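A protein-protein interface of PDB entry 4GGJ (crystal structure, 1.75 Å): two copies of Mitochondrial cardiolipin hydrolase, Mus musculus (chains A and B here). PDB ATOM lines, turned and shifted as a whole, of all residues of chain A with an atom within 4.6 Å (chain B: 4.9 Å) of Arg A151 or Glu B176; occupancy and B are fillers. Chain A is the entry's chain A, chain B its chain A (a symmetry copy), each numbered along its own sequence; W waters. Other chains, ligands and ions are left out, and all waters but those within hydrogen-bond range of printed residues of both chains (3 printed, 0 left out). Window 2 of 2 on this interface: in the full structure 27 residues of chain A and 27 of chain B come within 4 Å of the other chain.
The side-chain carboxylate of Glu A152 sits at hydrogen-bond distance from a ring nitrogen (ND1) of His B124, at 2.8 Å. The backbone NH (N) of His B124 sits at hydrogen-bond distance from the backbone carbonyl oxygen (O) of Arg A151 (3.0 Å). The backbone NH of His B125 sits at hydrogen-bond distance from the backbone carbonyl oxygen of Arg A151, at 3.4 Å. N of Arg A151 sits at hydrogen-bond distance from O of Tyr B122. The guanidinium group (NH2) of Arg A151 is in salt-bridge range of the side-chain carboxylate (OE1) of Glu B176 (2.6 Å).
The backbone carbonyl oxygen of Glu A152 sits at hydrogen-bond distance from the backbone NH of Phe A14, 2.9 Å away. A ring nitrogen (NE2) of His B125 lies within hydrogen-bond range of the side-chain carboxylate of Glu B169 (2.8 Å). ND2 of Asn A150 sits at hydrogen-bond distance from OE2 of Glu A152 (3.0 Å).
Among the printed residues, merely in contact across the chains: Glu A152 with His B125, Asn A150 with Tyr B122, Arg A151 with Ile B173 and Asn A149 with Tyr B122.
Of chain B, only Tyr B122 (2.7 Å), His B124 (3.0 Å), His B125 (3.4 Å), Ile B173 (3.7 Å) and Glu B176 (2.6 Å) come within 4 Å of Arg A151. Of the printed residues of chain B, Glu A152 touches His B124 and His B125. Printed residues of chain A within 4 Å of Tyr B122: Asn A149 (3.7 Å), Asn A150 (3.3 Å) and Arg A151 (2.7 Å). The nearest printed residue of chain B that does not touch Arg A151 is Glu B169 (4.1 Å). The nearest printed residue of chain A that does not touch Glu B176 is Pro A15 (8.1 Å). The nearest printed residue of chain A that does not touch Ile B173 is Glu A152 (6.9 Å).
Of the 6 printed residues of chain A, 4 touch a printed residue of chain B. Of the 12 printed residues of chain B, 5 touch a printed residue of chain A. Among the printed residues, Asp or Glu carboxylates within 4 Å of a Lys or Arg side-chain nitrogen of the other chain: Arg A151 with Glu B176.
No position is printed for both chains. Of the 9 pairs that touch across the chains among the printed residues, none has its exchanged pair printed and touching as well.
Water W3 bridges NE of Arg A151 (2.4 Å) and OE1 of Glu B176 (3.1 Å). Water W1 lies within hydrogen-bond range of the side-chain carboxylate of Glu A152 (2.6 Å) and a ring nitrogen (ND1) of His B124 (3.3 Å). Water W2 lies within hydrogen-bond range of the backbone carbonyl oxygen (O) of Phe A14, the side-chain carboxylate (OE2) of Glu B169 and the guanidinium group (NH1) of Arg A151.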
ATOM      1  N   PHE A  14      -8.130  -1.642 -21.117  1.00  0.00           N
ATOM      2  CA  PHE A  14      -8.810  -2.086 -19.926  1.00  0.00           C
ATOM      3  C   PHE A  14      -8.344  -3.511 -19.675  1.00  0.00           C
ATOM      4  O   PHE A  14      -7.873  -4.170 -20.593  1.00  0.00           O
ATOM      5  CB  PHE A  14     -10.325  -2.010 -20.158  1.00  0.00           C
ATOM      6  CG  PHE A  14     -10.839  -0.606 -20.279  1.00  0.00           C
ATOM      7  CD1 PHE A  14     -10.683   0.105 -21.472  1.00  0.00           C
ATOM      8  CD2 PHE A  14     -11.442   0.021 -19.209  1.00  0.00           C
ATOM      9  CE1 PHE A  14     -11.131   1.402 -21.593  1.00  0.00           C
ATOM     10  CE2 PHE A  14     -11.907   1.343 -19.334  1.00  0.00           C
ATOM     11  CZ  PHE A  14     -11.752   2.019 -20.541  1.00  0.00           C
ATOM     12  N   PRO A  15      -8.489  -4.024 -18.441  1.00  0.00           N
ATOM     13  CA  PRO A  15      -9.203  -3.453 -17.291  1.00  0.00           C
ATOM     14  C   PRO A  15      -8.610  -2.169 -16.726  1.00  0.00           C
ATOM     15  O   PRO A  15      -7.388  -1.986 -16.718  1.00  0.00           O
ATOM     16  CB  PRO A  15      -9.129  -4.555 -16.227  1.00  0.00           C
ATOM     17  CG  PRO A  15      -8.223  -5.573 -16.739  1.00  0.00           C
ATOM     18  CD  PRO A  15      -7.976  -5.378 -18.175  1.00  0.00           C
ATOM     19  N   ASN A 149     -12.803  -5.710 -15.353  1.00  0.00           N
ATOM     20  CA  ASN A 149     -12.369  -7.083 -15.521  1.00  0.00           C
ATOM     21  C   ASN A 149     -11.924  -7.515 -16.914  1.00  0.00           C
ATOM     22  O   ASN A 149     -11.180  -8.509 -17.024  1.00  0.00           O
ATOM     23  CB  ASN A 149     -13.489  -8.013 -15.052  1.00  0.00           C
ATOM     24  CG  ASN A 149     -13.785  -7.838 -13.587  1.00  0.00           C
ATOM     25  OD1 ASN A 149     -13.060  -8.362 -12.743  1.00  0.00           O
ATOM     26  ND2 ASN A 149     -14.825  -7.037 -13.270  1.00  0.00           N
ATOM     27  N   ASN A 150     -12.381  -6.828 -17.957  1.00  0.00           N
ATOM     28  CA  ASN A 150     -12.154  -7.319 -19.323  1.00  0.00           C
ATOM     29  C   ASN A 150     -10.974  -6.647 -19.974  1.00  0.00           C
ATOM     30  O   ASN A 150     -10.715  -5.477 -19.728  1.00  0.00           O
ATOM     31  CB  ASN A 150     -13.366  -7.062 -20.218  1.00  0.00           C
ATOM     32  CG  ASN A 150     -14.556  -7.924 -19.867  1.00  0.00           C
ATOM     33  OD1 ASN A 150     -14.501  -8.774 -18.975  1.00  0.00           O
ATOM     34  ND2 ASN A 150     -15.649  -7.728 -20.609  1.00  0.00           N
ATOM     35  N   ARG A 151     -10.290  -7.397 -20.834  1.00  0.00           N
ATOM     36  CA  ARG A 151      -9.348  -6.833 -21.757  1.00  0.00           C
ATOM     37  C   ARG A 151     -10.168  -6.195 -22.880  1.00  0.00           C
ATOM     38  O   ARG A 151     -10.971  -6.874 -23.532  1.00  0.00           O
ATOM     39  CB  ARG A 151      -8.445  -7.938 -22.309  1.00  0.00           C
ATOM     40  CG  ARG A 151      -7.654  -8.699 -21.248  1.00  0.00           C
ATOM     41  CD  ARG A 151      -6.514  -7.849 -20.666  1.00  0.00           C
ATOM     42  NE  ARG A 151      -5.274  -8.619 -20.537  1.00  0.00           N
ATOM     43  CZ  ARG A 151      -4.089  -8.126 -20.178  1.00  0.00           C
ATOM     44  NH1 ARG A 151      -3.943  -6.830 -19.897  1.00  0.00           N
ATOM     45  NH2 ARG A 151      -3.039  -8.941 -20.102  1.00  0.00           N
ATOM     46  N   GLU A 152     -10.016  -4.887 -23.033  1.00  0.00           N
ATOM     47  CA  GLU A 152     -10.789  -4.077 -23.975  1.00  0.00           C
ATOM     48  C   GLU A 152      -9.938  -2.922 -24.442  1.00  0.00           C
ATOM     49  O   GLU A 152      -8.957  -2.557 -23.772  1.00  0.00           O
ATOM     50  CB  GLU A 152     -12.005  -3.430 -23.302  1.00  0.00           C
ATOM     51  CG  GLU A 152     -12.896  -4.317 -22.445  1.00  0.00           C
ATOM     52  CD  GLU A 152     -14.048  -4.910 -23.195  1.00  0.00           C
ATOM     53  OE1 GLU A 152     -14.099  -4.792 -24.447  1.00  0.00           O
ATOM     54  OE2 GLU A 152     -14.906  -5.525 -22.528  1.00  0.00           O
ATOM     55  N   TYR B 122     -13.687 -12.388 -20.500  1.00  0.00           N
ATOM     56  CA  TYR B 122     -12.625 -11.458 -20.146  1.00  0.00           C
ATOM     57  C   TYR B 122     -11.826 -10.983 -21.324  1.00  0.00           C
ATOM     58  O   TYR B 122     -11.436  -9.822 -21.345  1.00  0.00           O
ATOM     59  CB  TYR B 122     -11.655 -12.021 -19.101  1.00  0.00           C
ATOM     60  CG  TYR B 122     -12.269 -12.369 -17.765  1.00  0.00           C
ATOM     61  CD1 TYR B 122     -13.271 -11.585 -17.182  1.00  0.00           C
ATOM     62  CD2 TYR B 122     -11.832 -13.495 -17.067  1.00  0.00           C
ATOM     63  CE1 TYR B 122     -13.820 -11.935 -15.932  1.00  0.00           C
ATOM     64  CE2 TYR B 122     -12.364 -13.831 -15.863  1.00  0.00           C
ATOM     65  CZ  TYR B 122     -13.359 -13.059 -15.294  1.00  0.00           C
ATOM     66  OH  TYR B 122     -13.851 -13.444 -14.077  1.00  0.00           O
ATOM     67  N   MET B 123     -11.546 -11.844 -22.303  1.00  0.00           N
ATOM     68  CA  MET B 123     -10.709 -11.392 -23.425  1.00  0.00           C
ATOM     69  C   MET B 123     -11.625 -10.850 -24.520  1.00  0.00           C
ATOM     70  O   MET B 123     -12.054 -11.583 -25.406  1.00  0.00           O
ATOM     71  CB  MET B 123      -9.811 -12.532 -23.930  1.00  0.00           C
ATOM     72  CG  MET B 123      -8.464 -12.035 -24.473  1.00  0.00           C
ATOM     73  SD  MET B 123      -8.592 -10.825 -25.778  1.00  0.00           S
ATOM     74  CE  MET B 123      -9.318 -11.771 -27.123  1.00  0.00           C
ATOM     75  N   HIS B 124     -11.916  -9.549 -24.446  1.00  0.00           N
ATOM     76  CA  HIS B 124     -13.012  -8.966 -25.220  1.00  0.00           C
ATOM     77  C   HIS B 124     -12.587  -8.086 -26.420  1.00  0.00           C
ATOM     78  O   HIS B 124     -13.435  -7.545 -27.136  1.00  0.00           O
ATOM     79  CB  HIS B 124     -13.929  -8.202 -24.256  1.00  0.00           C
ATOM     80  CG  HIS B 124     -15.326  -8.005 -24.763  1.00  0.00           C
ATOM     81  ND1 HIS B 124     -15.763  -6.807 -25.305  1.00  0.00           N
ATOM     82  CD2 HIS B 124     -16.398  -8.838 -24.785  1.00  0.00           C
ATOM     83  CE1 HIS B 124     -17.032  -6.918 -25.658  1.00  0.00           C
ATOM     84  NE2 HIS B 124     -17.441  -8.144 -25.360  1.00  0.00           N
ATOM     85  N   HIS B 125     -11.288  -7.991 -26.679  1.00  0.00           N
ATOM     86  CA  HIS B 125     -10.778  -7.356 -27.915  1.00  0.00           C
ATOM     87  C   HIS B 125     -11.320  -8.006 -29.205  1.00  0.00           C
ATOM     88  O   HIS B 125     -11.604  -9.216 -29.255  1.00  0.00           O
ATOM     89  CB  HIS B 125      -9.255  -7.462 -27.982  1.00  0.00           C
ATOM     90  CG  HIS B 125      -8.523  -6.628 -26.970  1.00  0.00           C
ATOM     91  ND1 HIS B 125      -8.638  -5.252 -26.905  1.00  0.00           N
ATOM     92  CD2 HIS B 125      -7.634  -6.975 -26.013  1.00  0.00           C
ATOM     93  CE1 HIS B 125      -7.857  -4.792 -25.942  1.00  0.00           C
ATOM     94  NE2 HIS B 125      -7.224  -5.813 -25.393  1.00  0.00           N
ATOM     95  N   GLU B 169       0.145  -4.645 -26.427  1.00  0.00           N
ATOM     96  CA  GLU B 169      -0.950  -5.267 -25.704  1.00  0.00           C
ATOM     97  C   GLU B 169      -1.051  -6.731 -26.122  1.00  0.00           C
ATOM     98  O   GLU B 169      -1.154  -7.633 -25.280  1.00  0.00           O
ATOM     99  CB  GLU B 169      -2.266  -4.499 -25.967  1.00  0.00           C
ATOM    100  CG  GLU B 169      -3.575  -5.183 -25.505  1.00  0.00           C
ATOM    101  CD  GLU B 169      -3.900  -5.023 -24.016  1.00  0.00           C
ATOM    102  OE1 GLU B 169      -3.046  -4.523 -23.238  1.00  0.00           O
ATOM    103  OE2 GLU B 169      -5.051  -5.391 -23.639  1.00  0.00           O
ATOM    104  N   ARG B 172       1.683  -8.814 -24.520  1.00  0.00           N
ATOM    105  CA  ARG B 172       1.439  -9.005 -23.080  1.00  0.00           C
ATOM    106  C   ARG B 172       0.469 -10.153 -22.849  1.00  0.00           C
ATOM    107  O   ARG B 172       0.709 -11.019 -22.002  1.00  0.00           O
ATOM    108  CB  ARG B 172       0.847  -7.732 -22.449  1.00  0.00           C
ATOM    109  CG  ARG B 172       1.875  -6.655 -22.112  1.00  0.00           C
ATOM    110  CD  ARG B 172       1.263  -5.580 -21.200  1.00  0.00           C
ATOM    111  NE  ARG B 172       0.183  -4.824 -21.839  1.00  0.00           N
ATOM    112  CZ  ARG B 172       0.338  -3.678 -22.511  1.00  0.00           C
ATOM    113  NH1 ARG B 172       1.544  -3.137 -22.650  1.00  0.00           N
ATOM    114  NH2 ARG B 172      -0.720  -3.061 -23.049  1.00  0.00           N
ATOM    115  N   ILE B 173      -0.630 -10.134 -23.595  1.00  0.00           N
ATOM    116  CA  ILE B 173      -1.661 -11.178 -23.483  1.00  0.00           C
ATOM    117  C   ILE B 173      -1.095 -12.533 -23.977  1.00  0.00           C
ATOM    118  O   ILE B 173      -1.341 -13.572 -23.357  1.00  0.00           O
ATOM    119  CB  ILE B 173      -2.961 -10.815 -24.225  1.00  0.00           C
ATOM    120  CG1 ILE B 173      -3.527  -9.466 -23.728  1.00  0.00           C
ATOM    121  CG2 ILE B 173      -4.034 -11.913 -24.005  1.00  0.00           C
ATOM    122  CD1 ILE B 173      -4.684  -8.919 -24.567  1.00  0.00           C
ATOM    123  N   TRP B 174      -0.354 -12.507 -25.085  1.00  0.00           N
ATOM    124  CA  TRP B 174       0.313 -13.705 -25.641  1.00  0.00           C
ATOM    125  C   TRP B 174       1.197 -14.416 -24.612  1.00  0.00           C
ATOM    126  O   TRP B 174       1.142 -15.641 -24.451  1.00  0.00           O
ATOM    127  CB  TRP B 174       1.157 -13.321 -26.883  1.00  0.00           C
ATOM    128  CG  TRP B 174       1.733 -14.504 -27.629  1.00  0.00           C
ATOM    129  CD1 TRP B 174       3.035 -14.898 -27.671  1.00  0.00           C
ATOM    130  CD2 TRP B 174       1.005 -15.438 -28.426  1.00  0.00           C
ATOM    131  NE1 TRP B 174       3.166 -16.040 -28.448  1.00  0.00           N
ATOM    132  CE2 TRP B 174       1.927 -16.379 -28.925  1.00  0.00           C
ATOM    133  CE3 TRP B 174      -0.342 -15.571 -28.760  1.00  0.00           C
ATOM    134  CZ2 TRP B 174       1.538 -17.443 -29.734  1.00  0.00           C
ATOM    135  CZ3 TRP B 174      -0.723 -16.618 -29.580  1.00  0.00           C
ATOM    136  CH2 TRP B 174       0.209 -17.540 -30.049  1.00  0.00           C
ATOM    137  N   GLU B 175       2.014 -13.646 -23.910  1.00  0.00           N
ATOM    138  CA  GLU B 175       2.895 -14.212 -22.903  1.00  0.00           C
ATOM    139  C   GLU B 175       2.136 -14.681 -21.658  1.00  0.00           C
ATOM    140  O   GLU B 175       2.467 -15.702 -21.082  1.00  0.00           O
ATOM    141  CB  GLU B 175       3.972 -13.208 -22.524  1.00  0.00           C
ATOM    142  CG  GLU B 175       4.924 -12.898 -23.688  1.00  0.00           C
ATOM    143  CD  GLU B 175       5.722 -14.107 -24.166  1.00  0.00           C
ATOM    144  OE1 GLU B 175       6.103 -14.954 -23.317  1.00  0.00           O
ATOM    145  OE2 GLU B 175       5.993 -14.208 -25.390  1.00  0.00           O
ATOM    146  N   GLU B 176       1.099 -13.943 -21.267  1.00  0.00           N
ATOM    147  CA  GLU B 176       0.288 -14.325 -20.123  1.00  0.00           C
ATOM    148  C   GLU B 176      -0.364 -15.691 -20.329  1.00  0.00           C
ATOM    149  O   GLU B 176      -0.500 -16.456 -19.378  1.00  0.00           O
ATOM    150  CB  GLU B 176      -0.785 -13.274 -19.880  1.00  0.00           C
ATOM    151  CG  GLU B 176      -1.586 -13.460 -18.617  1.00  0.00           C
ATOM    152  CD  GLU B 176      -2.679 -12.400 -18.472  1.00  0.00           C
ATOM    153  OE1 GLU B 176      -2.480 -11.253 -18.936  1.00  0.00           O
ATOM    154  OE2 GLU B 176      -3.737 -12.721 -17.887  1.00  0.00           O
ATOM    155  N   PHE B 177      -0.759 -15.984 -21.569  1.00  0.00           N
ATOM    156  CA  PHE B 177      -1.496 -17.213 -21.894  1.00  0.00           C
ATOM    157  C   PHE B 177      -0.596 -18.342 -22.415  1.00  0.00           C
ATOM    158  O   PHE B 177      -1.102 -19.335 -22.951  1.00  0.00           O
ATOM    159  CB  PHE B 177      -2.576 -16.943 -22.957  1.00  0.00           C
ATOM    160  CG  PHE B 177      -3.668 -15.983 -22.536  1.00  0.00           C
ATOM    161  CD1 PHE B 177      -3.773 -15.507 -21.240  1.00  0.00           C
ATOM    162  CD2 PHE B 177      -4.619 -15.586 -23.462  1.00  0.00           C
ATOM    163  CE1 PHE B 177      -4.804 -14.633 -20.886  1.00  0.00           C
ATOM    164  CE2 PHE B 177      -5.648 -14.716 -23.115  1.00  0.00           C
ATOM    165  CZ  PHE B 177      -5.740 -14.250 -21.826  1.00  0.00           C
ATOM    166  N   ASP B 178       0.717 -18.193 -22.269  1.00  0.00           N
ATOM    167  CA  ASP B 178       1.658 -19.225 -22.696  1.00  0.00           C
ATOM    168  C   ASP B 178       1.321 -20.506 -21.929  1.00  0.00           C
ATOM    169  O   ASP B 178       1.438 -20.530 -20.701  1.00  0.00           O
ATOM    170  CB  ASP B 178       3.089 -18.788 -22.407  1.00  0.00           C
ATOM    171  CG  ASP B 178       4.144 -19.765 -22.938  1.00  0.00           C
ATOM    172  OD1 ASP B 178       3.816 -20.895 -23.368  1.00  0.00           O
ATOM    173  OD2 ASP B 178       5.330 -19.387 -22.908  1.00  0.00           O
HETATM  174  O   HOH W   1     -17.400  -5.178 -22.960  1.00  0.00           O
HETATM  175  O   HOH W   2      -5.336  -4.754 -20.999  1.00  0.00           O
HETATM  176  O   HOH W   3      -5.437 -10.942 -19.885  1.00  0.00           O
